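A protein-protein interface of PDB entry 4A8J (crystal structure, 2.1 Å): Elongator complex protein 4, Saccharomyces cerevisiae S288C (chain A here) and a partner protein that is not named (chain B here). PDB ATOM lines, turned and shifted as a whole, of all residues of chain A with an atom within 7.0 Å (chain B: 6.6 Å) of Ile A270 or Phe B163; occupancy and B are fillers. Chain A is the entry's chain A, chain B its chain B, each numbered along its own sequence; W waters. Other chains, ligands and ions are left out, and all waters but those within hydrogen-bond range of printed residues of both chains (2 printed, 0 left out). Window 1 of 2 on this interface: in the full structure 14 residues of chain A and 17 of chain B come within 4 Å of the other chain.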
ATOM      1  N   SER A  49      11.053 -23.551 -25.213  1.00  0.00           N
ATOM      2  CA  SER A  49      12.339 -24.241 -25.007  1.00  0.00           C
ATOM      3  C   SER A  49      13.322 -23.432 -24.166  1.00  0.00           C
ATOM      4  O   SER A  49      12.925 -22.496 -23.472  1.00  0.00           O
ATOM      5  CB  SER A  49      12.986 -24.687 -26.330  1.00  0.00           C
ATOM      6  OG  SER A  49      13.511 -23.587 -27.062  1.00  0.00           O
ATOM      7  N   THR A  50      14.601 -23.805 -24.240  1.00  0.00           N
ATOM      8  CA  THR A  50      15.633 -23.225 -23.394  1.00  0.00           C
ATOM      9  C   THR A  50      16.518 -22.212 -24.136  1.00  0.00           C
ATOM     10  O   THR A  50      17.433 -21.630 -23.553  1.00  0.00           O
ATOM     11  CB  THR A  50      16.510 -24.337 -22.807  1.00  0.00           C
ATOM     12  OG1 THR A  50      16.973 -25.147 -23.887  1.00  0.00           O
ATOM     13  CG2 THR A  50      15.676 -25.212 -21.830  1.00  0.00           C
ATOM     14  N   GLU A  52      17.390 -18.618 -26.198  1.00  0.00           N
ATOM     15  CA  GLU A  52      17.024 -17.220 -25.962  1.00  0.00           C
ATOM     16  C   GLU A  52      17.160 -16.346 -27.216  1.00  0.00           C
ATOM     17  O   GLU A  52      17.843 -15.315 -27.214  1.00  0.00           O
ATOM     18  CB  GLU A  52      17.821 -16.637 -24.781  1.00  0.00           C
ATOM     19  CG  GLU A  52      17.532 -17.330 -23.445  1.00  0.00           C
ATOM     20  CD  GLU A  52      18.123 -16.607 -22.239  1.00  0.00           C
ATOM     21  OE1 GLU A  52      19.360 -16.685 -22.040  1.00  0.00           O
ATOM     22  OE2 GLU A  52      17.343 -15.965 -21.491  1.00  0.00           O
ATOM     23  N   LEU A 227      10.443 -12.309 -15.530  1.00  0.00           N
ATOM     24  CA  LEU A 227      10.191 -13.475 -14.673  1.00  0.00           C
ATOM     25  C   LEU A 227      11.237 -14.591 -14.764  1.00  0.00           C
ATOM     26  O   LEU A 227      10.970 -15.737 -14.394  1.00  0.00           O
ATOM     27  CB  LEU A 227       8.789 -14.060 -14.899  1.00  0.00           C
ATOM     28  CG  LEU A 227       7.642 -13.195 -14.347  1.00  0.00           C
ATOM     29  CD1 LEU A 227       6.311 -13.739 -14.810  1.00  0.00           C
ATOM     30  CD2 LEU A 227       7.706 -13.135 -12.815  1.00  0.00           C
ATOM     31  N   HIS A 228      12.427 -14.274 -15.234  1.00  0.00           N
ATOM     32  CA  HIS A 228      13.495 -15.257 -15.157  1.00  0.00           C
ATOM     33  C   HIS A 228      13.781 -15.523 -13.675  1.00  0.00           C
ATOM     34  O   HIS A 228      14.056 -14.588 -12.922  1.00  0.00           O
ATOM     35  CB  HIS A 228      14.747 -14.724 -15.848  1.00  0.00           C
ATOM     36  CG  HIS A 228      15.772 -15.779 -16.099  1.00  0.00           C
ATOM     37  ND1 HIS A 228      16.438 -16.411 -15.078  1.00  0.00           N
ATOM     38  CD2 HIS A 228      16.238 -16.307 -17.256  1.00  0.00           C
ATOM     39  CE1 HIS A 228      17.282 -17.297 -15.594  1.00  0.00           C
ATOM     40  NE2 HIS A 228      17.183 -17.252 -16.905  1.00  0.00           N
ATOM     41  N   PRO A 229      13.746 -16.801 -13.245  1.00  0.00           N
ATOM     42  CA  PRO A 229      13.837 -17.084 -11.801  1.00  0.00           C
ATOM     43  C   PRO A 229      15.231 -16.833 -11.193  1.00  0.00           C
ATOM     44  O   PRO A 229      15.398 -16.874  -9.982  1.00  0.00           O
ATOM     45  CB  PRO A 229      13.477 -18.582 -11.698  1.00  0.00           C
ATOM     46  CG  PRO A 229      13.060 -19.014 -13.084  1.00  0.00           C
ATOM     47  CD  PRO A 229      13.648 -18.028 -14.054  1.00  0.00           C
ATOM     48  N   ALA A 230      16.225 -16.601 -12.020  1.00  0.00           N
ATOM     49  CA  ALA A 230      17.539 -16.255 -11.505  1.00  0.00           C
ATOM     50  C   ALA A 230      17.536 -14.789 -11.099  1.00  0.00           C
ATOM     51  O   ALA A 230      18.387 -14.342 -10.339  1.00  0.00           O
ATOM     52  CB  ALA A 230      18.586 -16.499 -12.559  1.00  0.00           C
ATOM     53  N   PHE A 237       6.314 -13.578  -7.942  1.00  0.00           N
ATOM     54  CA  PHE A 237       5.439 -14.453  -8.719  1.00  0.00           C
ATOM     55  C   PHE A 237       3.992 -14.463  -8.211  1.00  0.00           C
ATOM     56  O   PHE A 237       3.105 -15.034  -8.854  1.00  0.00           O
ATOM     57  CB  PHE A 237       5.998 -15.879  -8.770  1.00  0.00           C
ATOM     58  CG  PHE A 237       7.117 -16.068  -9.764  1.00  0.00           C
ATOM     59  CD1 PHE A 237       8.381 -15.562  -9.514  1.00  0.00           C
ATOM     60  CD2 PHE A 237       6.899 -16.763 -10.947  1.00  0.00           C
ATOM     61  CE1 PHE A 237       9.418 -15.735 -10.428  1.00  0.00           C
ATOM     62  CE2 PHE A 237       7.929 -16.951 -11.865  1.00  0.00           C
ATOM     63  CZ  PHE A 237       9.193 -16.435 -11.601  1.00  0.00           C
ATOM     64  N   SER A 267      10.562 -16.461 -21.327  1.00  0.00           N
ATOM     65  CA  SER A 267      10.629 -17.912 -21.551  1.00  0.00           C
ATOM     66  C   SER A 267       9.398 -18.549 -20.922  1.00  0.00           C
ATOM     67  O   SER A 267       9.266 -18.581 -19.706  1.00  0.00           O
ATOM     68  CB  SER A 267      11.885 -18.498 -20.887  1.00  0.00           C
ATOM     69  OG  SER A 267      13.050 -17.989 -21.510  1.00  0.00           O
ATOM     70  N   ILE A 268       8.502 -19.089 -21.732  1.00  0.00           N
ATOM     71  CA  ILE A 268       7.223 -19.461 -21.176  1.00  0.00           C
ATOM     72  C   ILE A 268       7.152 -20.886 -20.629  1.00  0.00           C
ATOM     73  O   ILE A 268       6.156 -21.251 -20.015  1.00  0.00           O
ATOM     74  CB  ILE A 268       6.082 -19.245 -22.167  1.00  0.00           C
ATOM     75  CG1 ILE A 268       6.285 -20.078 -23.428  1.00  0.00           C
ATOM     76  CG2 ILE A 268       5.954 -17.780 -22.510  1.00  0.00           C
ATOM     77  CD1 ILE A 268       5.042 -20.081 -24.303  1.00  0.00           C
ATOM     78  N   ASP A 269       8.184 -21.699 -20.839  1.00  0.00           N
ATOM     79  CA  ASP A 269       8.061 -23.112 -20.467  1.00  0.00           C
ATOM     80  C   ASP A 269       7.862 -23.340 -18.969  1.00  0.00           C
ATOM     81  O   ASP A 269       7.142 -24.259 -18.580  1.00  0.00           O
ATOM     82  CB  ASP A 269       9.216 -23.955 -21.027  1.00  0.00           C
ATOM     83  CG  ASP A 269       9.026 -24.280 -22.509  1.00  0.00           C
ATOM     84  OD1 ASP A 269       7.917 -24.030 -23.034  1.00  0.00           O
ATOM     85  OD2 ASP A 269       9.974 -24.788 -23.147  1.00  0.00           O
ATOM     86  N   ILE A 270       8.493 -22.512 -18.141  1.00  0.00           N
ATOM     87  CA  ILE A 270       8.299 -22.595 -16.702  1.00  0.00           C
ATOM     88  C   ILE A 270       7.210 -21.655 -16.144  1.00  0.00           C
ATOM     89  O   ILE A 270       7.072 -21.528 -14.941  1.00  0.00           O
ATOM     90  CB  ILE A 270       9.604 -22.305 -15.953  1.00  0.00           C
ATOM     91  CG1 ILE A 270      10.076 -20.887 -16.263  1.00  0.00           C
ATOM     92  CG2 ILE A 270      10.669 -23.337 -16.317  1.00  0.00           C
ATOM     93  CD1 ILE A 270      10.473 -20.109 -15.024  1.00  0.00           C
ATOM     94  N   ILE A 271       6.453 -20.985 -17.008  1.00  0.00           N
ATOM     95  CA  ILE A 271       5.369 -20.103 -16.530  1.00  0.00           C
ATOM     96  C   ILE A 271       4.092 -20.931 -16.378  1.00  0.00           C
ATOM     97  O   ILE A 271       3.668 -21.580 -17.336  1.00  0.00           O
ATOM     98  CB  ILE A 271       5.085 -18.953 -17.524  1.00  0.00           C
ATOM     99  CG1 ILE A 271       6.343 -18.110 -17.766  1.00  0.00           C
ATOM    100  CG2 ILE A 271       3.934 -18.048 -17.017  1.00  0.00           C
ATOM    101  CD1 ILE A 271       6.918 -17.500 -16.496  1.00  0.00           C
ATOM    102  N   THR A 272       3.465 -20.922 -15.201  1.00  0.00           N
ATOM    103  CA  THR A 272       2.228 -21.684 -15.030  1.00  0.00           C
ATOM    104  C   THR A 272       1.160 -21.080 -15.926  1.00  0.00           C
ATOM    105  O   THR A 272       1.051 -19.864 -16.025  1.00  0.00           O
ATOM    106  CB  THR A 272       1.708 -21.642 -13.587  1.00  0.00           C
ATOM    107  OG1 THR A 272       1.151 -20.344 -13.333  1.00  0.00           O
ATOM    108  CG2 THR A 272       2.827 -21.893 -12.610  1.00  0.00           C
ATOM    109  N   PRO A 273       0.348 -21.928 -16.562  1.00  0.00           N
ATOM    110  CA  PRO A 273      -0.691 -21.509 -17.514  1.00  0.00           C
ATOM    111  C   PRO A 273      -1.538 -20.293 -17.097  1.00  0.00           C
ATOM    112  O   PRO A 273      -1.735 -19.378 -17.903  1.00  0.00           O
ATOM    113  CB  PRO A 273      -1.567 -22.758 -17.627  1.00  0.00           C
ATOM    114  CG  PRO A 273      -0.593 -23.875 -17.462  1.00  0.00           C
ATOM    115  CD  PRO A 273       0.390 -23.396 -16.411  1.00  0.00           C
ATOM    116  N   LEU A 275      -0.935 -17.869 -15.115  1.00  0.00           N
ATOM    117  CA  LEU A 275      -0.139 -16.656 -15.037  1.00  0.00           C
ATOM    118  C   LEU A 275       0.169 -16.199 -16.462  1.00  0.00           C
ATOM    119  O   LEU A 275       0.170 -15.006 -16.786  1.00  0.00           O
ATOM    120  CB  LEU A 275       1.159 -16.907 -14.235  1.00  0.00           C
ATOM    121  CG  LEU A 275       2.161 -15.742 -14.229  1.00  0.00           C
ATOM    122  CD1 LEU A 275       1.429 -14.500 -13.732  1.00  0.00           C
ATOM    123  CD2 LEU A 275       3.416 -16.031 -13.353  1.00  0.00           C
ATOM    124  N   LEU B  26      21.790 -32.419 -12.882  1.00  0.00           N
ATOM    125  CA  LEU B  26      20.638 -32.799 -12.079  1.00  0.00           C
ATOM    126  C   LEU B  26      20.294 -34.238 -12.424  1.00  0.00           C
ATOM    127  O   LEU B  26      20.072 -34.550 -13.587  1.00  0.00           O
ATOM    128  CB  LEU B  26      19.458 -31.888 -12.404  1.00  0.00           C
ATOM    129  CG  LEU B  26      18.106 -32.267 -11.802  1.00  0.00           C
ATOM    130  CD1 LEU B  26      18.108 -32.014 -10.270  1.00  0.00           C
ATOM    131  CD2 LEU B  26      16.937 -31.537 -12.510  1.00  0.00           C
ATOM    132  N   ASN B 153       2.330 -18.239  -8.196  1.00  0.00           N
ATOM    133  CA  ASN B 153       2.601 -18.846  -9.483  1.00  0.00           C
ATOM    134  C   ASN B 153       4.047 -19.297  -9.651  1.00  0.00           C
ATOM    135  O   ASN B 153       4.503 -19.519 -10.773  1.00  0.00           O
ATOM    136  CB  ASN B 153       2.231 -17.835 -10.554  1.00  0.00           C
ATOM    137  CG  ASN B 153       0.785 -17.401 -10.426  1.00  0.00           C
ATOM    138  OD1 ASN B 153      -0.133 -18.214 -10.617  1.00  0.00           O
ATOM    139  ND2 ASN B 153       0.570 -16.135 -10.056  1.00  0.00           N
ATOM    140  N   TYR B 154       4.771 -19.425  -8.547  1.00  0.00           N
ATOM    141  CA  TYR B 154       6.158 -19.876  -8.620  1.00  0.00           C
ATOM    142  C   TYR B 154       6.167 -21.311  -9.133  1.00  0.00           C
ATOM    143  O   TYR B 154       5.321 -22.118  -8.746  1.00  0.00           O
ATOM    144  CB  TYR B 154       6.823 -19.806  -7.246  1.00  0.00           C
ATOM    145  CG  TYR B 154       8.340 -19.687  -7.337  1.00  0.00           C
ATOM    146  CD1 TYR B 154       8.933 -18.591  -7.967  1.00  0.00           C
ATOM    147  CD2 TYR B 154       9.169 -20.662  -6.799  1.00  0.00           C
ATOM    148  CE1 TYR B 154      10.319 -18.469  -8.057  1.00  0.00           C
ATOM    149  CE2 TYR B 154      10.565 -20.557  -6.881  1.00  0.00           C
ATOM    150  CZ  TYR B 154      11.132 -19.465  -7.511  1.00  0.00           C
ATOM    151  OH  TYR B 154      12.499 -19.356  -7.590  1.00  0.00           O
ATOM    152  N   PRO B 155       7.106 -21.635 -10.022  1.00  0.00           N
ATOM    153  CA  PRO B 155       7.180 -23.015 -10.534  1.00  0.00           C
ATOM    154  C   PRO B 155       7.402 -24.033  -9.417  1.00  0.00           C
ATOM    155  O   PRO B 155       8.014 -23.721  -8.388  1.00  0.00           O
ATOM    156  CB  PRO B 155       8.399 -22.991 -11.477  1.00  0.00           C
ATOM    157  CG  PRO B 155       9.195 -21.753 -11.077  1.00  0.00           C
ATOM    158  CD  PRO B 155       8.151 -20.762 -10.583  1.00  0.00           C
ATOM    159  N   ASP B 156       6.889 -25.241  -9.619  1.00  0.00           N
ATOM    160  CA  ASP B 156       7.145 -26.346  -8.726  1.00  0.00           C
ATOM    161  C   ASP B 156       8.629 -26.697  -8.794  1.00  0.00           C
ATOM    162  O   ASP B 156       9.353 -26.257  -9.699  1.00  0.00           O
ATOM    163  CB  ASP B 156       6.262 -27.549  -9.104  1.00  0.00           C
ATOM    164  CG  ASP B 156       6.473 -27.988 -10.536  1.00  0.00           C
ATOM    165  OD1 ASP B 156       7.421 -28.748 -10.784  1.00  0.00           O
ATOM    166  OD2 ASP B 156       5.707 -27.553 -11.426  1.00  0.00           O
ATOM    167  N   LEU B 158      10.500 -29.403  -9.359  1.00  0.00           N
ATOM    168  CA  LEU B 158      11.072 -30.164 -10.457  1.00  0.00           C
ATOM    169  C   LEU B 158      11.184 -29.274 -11.696  1.00  0.00           C
ATOM    170  O   LEU B 158      12.226 -29.234 -12.363  1.00  0.00           O
ATOM    171  CB  LEU B 158      10.226 -31.404 -10.749  1.00  0.00           C
ATOM    172  CG  LEU B 158      10.663 -32.195 -11.984  1.00  0.00           C
ATOM    173  CD1 LEU B 158      12.094 -32.688 -11.836  1.00  0.00           C
ATOM    174  CD2 LEU B 158       9.727 -33.353 -12.265  1.00  0.00           C
ATOM    175  N   THR B 159      10.110 -28.539 -11.995  1.00  0.00           N
ATOM    176  CA  THR B 159      10.118 -27.640 -13.141  1.00  0.00           C
ATOM    177  C   THR B 159      11.287 -26.643 -13.069  1.00  0.00           C
ATOM    178  O   THR B 159      12.010 -26.424 -14.046  1.00  0.00           O
ATOM    179  CB  THR B 159       8.788 -26.874 -13.247  1.00  0.00           C
ATOM    180  OG1 THR B 159       7.715 -27.808 -13.431  1.00  0.00           O
ATOM    181  CG2 THR B 159       8.833 -25.938 -14.423  1.00  0.00           C
ATOM    182  N   LEU B 160      11.485 -26.058 -11.891  1.00  0.00           N
ATOM    183  CA  LEU B 160      12.526 -25.065 -11.666  1.00  0.00           C
ATOM    184  C   LEU B 160      13.921 -25.691 -11.773  1.00  0.00           C
ATOM    185  O   LEU B 160      14.798 -25.186 -12.490  1.00  0.00           O
ATOM    186  CB  LEU B 160      12.329 -24.437 -10.279  1.00  0.00           C
ATOM    187  CG  LEU B 160      13.427 -23.477  -9.832  1.00  0.00           C
ATOM    188  CD1 LEU B 160      13.506 -22.221 -10.775  1.00  0.00           C
ATOM    189  CD2 LEU B 160      13.198 -23.072  -8.394  1.00  0.00           C
ATOM    190  N   LEU B 161      14.119 -26.807 -11.077  1.00  0.00           N
ATOM    191  CA  LEU B 161      15.389 -27.527 -11.135  1.00  0.00           C
ATOM    192  C   LEU B 161      15.781 -27.845 -12.567  1.00  0.00           C
ATOM    193  O   LEU B 161      16.917 -27.621 -12.969  1.00  0.00           O
ATOM    194  CB  LEU B 161      15.321 -28.823 -10.316  1.00  0.00           C
ATOM    195  CG  LEU B 161      15.357 -28.586  -8.812  1.00  0.00           C
ATOM    196  CD1 LEU B 161      15.158 -29.895  -8.075  1.00  0.00           C
ATOM    197  CD2 LEU B 161      16.701 -27.911  -8.438  1.00  0.00           C
ATOM    198  N   GLN B 162      14.840 -28.369 -13.339  1.00  0.00           N
ATOM    199  CA  GLN B 162      15.140 -28.732 -14.717  1.00  0.00           C
ATOM    200  C   GLN B 162      15.484 -27.490 -15.540  1.00  0.00           C
ATOM    201  O   GLN B 162      16.295 -27.555 -16.461  1.00  0.00           O
ATOM    202  CB  GLN B 162      13.963 -29.498 -15.342  1.00  0.00           C
ATOM    203  CG  GLN B 162      13.840 -30.927 -14.832  1.00  0.00           C
ATOM    204  CD  GLN B 162      12.984 -31.782 -15.737  1.00  0.00           C
ATOM    205  OE1 GLN B 162      13.481 -32.683 -16.422  1.00  0.00           O
ATOM    206  NE2 GLN B 162      11.697 -31.486 -15.774  1.00  0.00           N
ATOM    207  N   PHE B 163      14.876 -26.361 -15.188  1.00  0.00           N
ATOM    208  CA  PHE B 163      15.137 -25.109 -15.887  1.00  0.00           C
ATOM    209  C   PHE B 163      16.555 -24.598 -15.584  1.00  0.00           C
ATOM    210  O   PHE B 163      17.255 -24.122 -16.469  1.00  0.00           O
ATOM    211  CB  PHE B 163      14.101 -24.031 -15.507  1.00  0.00           C
ATOM    212  CG  PHE B 163      14.311 -22.725 -16.235  1.00  0.00           C
ATOM    213  CD1 PHE B 163      13.770 -22.531 -17.494  1.00  0.00           C
ATOM    214  CD2 PHE B 163      15.082 -21.714 -15.675  1.00  0.00           C
ATOM    215  CE1 PHE B 163      13.965 -21.333 -18.189  1.00  0.00           C
ATOM    216  CE2 PHE B 163      15.292 -20.521 -16.358  1.00  0.00           C
ATOM    217  CZ  PHE B 163      14.732 -20.330 -17.619  1.00  0.00           C
ATOM    218  N   MET B 164      16.965 -24.695 -14.325  1.00  0.00           N
ATOM    219  CA  MET B 164      18.273 -24.219 -13.888  1.00  0.00           C
ATOM    220  C   MET B 164      19.429 -25.150 -14.277  1.00  0.00           C
ATOM    221  O   MET B 164      20.578 -24.738 -14.308  1.00  0.00           O
ATOM    222  CB  MET B 164      18.252 -24.044 -12.364  1.00  0.00           C
ATOM    223  CG  MET B 164      17.182 -23.054 -11.875  1.00  0.00           C
ATOM    224  SD  MET B 164      17.555 -21.213 -12.556  1.00  0.00           S
ATOM    225  CE  MET B 164      19.192 -20.940 -11.466  1.00  0.00           C
ATOM    226  N   ALA B 165      19.131 -26.408 -14.567  1.00  0.00           N
ATOM    227  CA  ALA B 165      20.191 -27.396 -14.762  1.00  0.00           C
ATOM    228  C   ALA B 165      20.852 -27.192 -16.106  1.00  0.00           C
ATOM    229  O   ALA B 165      20.190 -26.827 -17.071  1.00  0.00           O
ATOM    230  CB  ALA B 165      19.641 -28.786 -14.677  1.00  0.00           C
ATOM    231  N   THR B 166      22.162 -27.440 -16.158  1.00  0.00           N
ATOM    232  CA  THR B 166      22.893 -27.412 -17.422  1.00  0.00           C
ATOM    233  C   THR B 166      22.914 -28.807 -18.034  1.00  0.00           C
ATOM    234  O   THR B 166      23.032 -28.961 -19.239  1.00  0.00           O
ATOM    235  CB  THR B 166      24.330 -26.872 -17.243  1.00  0.00           C
ATOM    236  OG1 THR B 166      24.968 -27.536 -16.148  1.00  0.00           O
ATOM    237  CG2 THR B 166      24.290 -25.380 -16.951  1.00  0.00           C
ATOM    238  N   ILE B 168      20.767 -32.727 -17.518  1.00  0.00           N
ATOM    239  CA  ILE B 168      19.802 -33.551 -16.791  1.00  0.00           C
ATOM    240  C   ILE B 168      20.034 -35.002 -17.146  1.00  0.00           C
ATOM    241  O   ILE B 168      20.141 -35.342 -18.320  1.00  0.00           O
ATOM    242  CB  ILE B 168      18.346 -33.212 -17.174  1.00  0.00           C
ATOM    243  CG1 ILE B 168      18.071 -31.712 -16.979  1.00  0.00           C
ATOM    244  CG2 ILE B 168      17.326 -34.065 -16.357  1.00  0.00           C
ATOM    245  CD1 ILE B 168      16.743 -31.251 -17.591  1.00  0.00           C
ATOM    246  N   LYS B 209      22.313 -29.425 -22.242  1.00  0.00           N
ATOM    247  CA  LYS B 209      21.942 -28.079 -22.629  1.00  0.00           C
ATOM    248  C   LYS B 209      23.194 -27.377 -23.117  1.00  0.00           C
ATOM    249  O   LYS B 209      24.037 -26.977 -22.304  1.00  0.00           O
ATOM    250  CB  LYS B 209      21.322 -27.338 -21.446  1.00  0.00           C
ATOM    251  CG  LYS B 209      20.822 -25.941 -21.788  1.00  0.00           C
ATOM    252  CD  LYS B 209      19.821 -25.469 -20.738  1.00  0.00           C
ATOM    253  CE  LYS B 209      20.261 -24.166 -20.070  1.00  0.00           C
ATOM    254  NZ  LYS B 209      20.197 -24.261 -18.573  1.00  0.00           N
HETATM  255  O   HOH W   1      13.412 -16.996  -8.249  1.00  0.00           O
HETATM  256  O   HOH W   2       5.110 -19.649 -13.358  1.00  0.00           O
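Water W1 lies within hydrogen-bond range of the side-chain hydroxyl (OH) of Tyr B154 (2.6 Å) and the backbone carbonyl oxygen (O) of Pro A229 (2.6 Å).
Water W2 lies within hydrogen-bond range of O of Asn B153 (2.7 Å), N of Thr A272 (2.8 Å) and O of Ile A270 (3.1 Å).
Hydrophobic or aromatic side chains of chain A that line the printed part of chain B: His A228, Pro A229, Phe A237, Ile A270 and Leu A275.
Among the printed residues, 10 pairs touch across the chains.
Among the printed residues, no Asp or Glu carboxylate lies within 4 Å of a Lys or Arg side-chain nitrogen of the other chain.
Of the printed residues of chain B, Ile A270 touches Pro B155, Thr B159 and Phe B163.
Phe B163 touches just these residues of chain A: His A228 (3.8 Å), Pro A229 (3.8 Å) and Ile A270 (3.4 Å).
Of the printed residues of chain B, Thr A272 touches Asn B153 (3.4 Å).
Printed residues of chain B within 4 Å of Leu A275: Asn B153.
Of the printed residues of chain A, Leu B160 touches Pro A229 (3.8 Å).
Glu A52 touches none of the printed residues of chain B.
The nearest printed residue of chain B that does not touch Thr A272 is Tyr B154 (4.6 Å).
The backbone carbonyl oxygen of Phe A237 sits at hydrogen-bond distance from the side-chain amide nitrogen of Asn B153 (3.0 Å).
OD1 of Asp B156 sits at hydrogen-bond distance from OG1 of Thr B159, 2.8 Å away.
ND1 of His A228 sits at hydrogen-bond distance from N of Ala A230.
Among the printed residues, pairs that only touch across the chains: His A228 with Phe B163 (3.8 Å), Pro A229 with Leu B160 (3.8 Å), Pro A229 with Phe B163 (3.8 Å), Phe A237 with Tyr B154 (3.4 Å), Ile A270 with Pro B155 (3.99 Å), Ile A270 with Thr B159 (3.7 Å), Ile A270 with Phe B163 (3.4 Å), Thr A272 with Asn B153 (3.4 Å) and Leu A275 with Asn B153 (3.5 Å).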
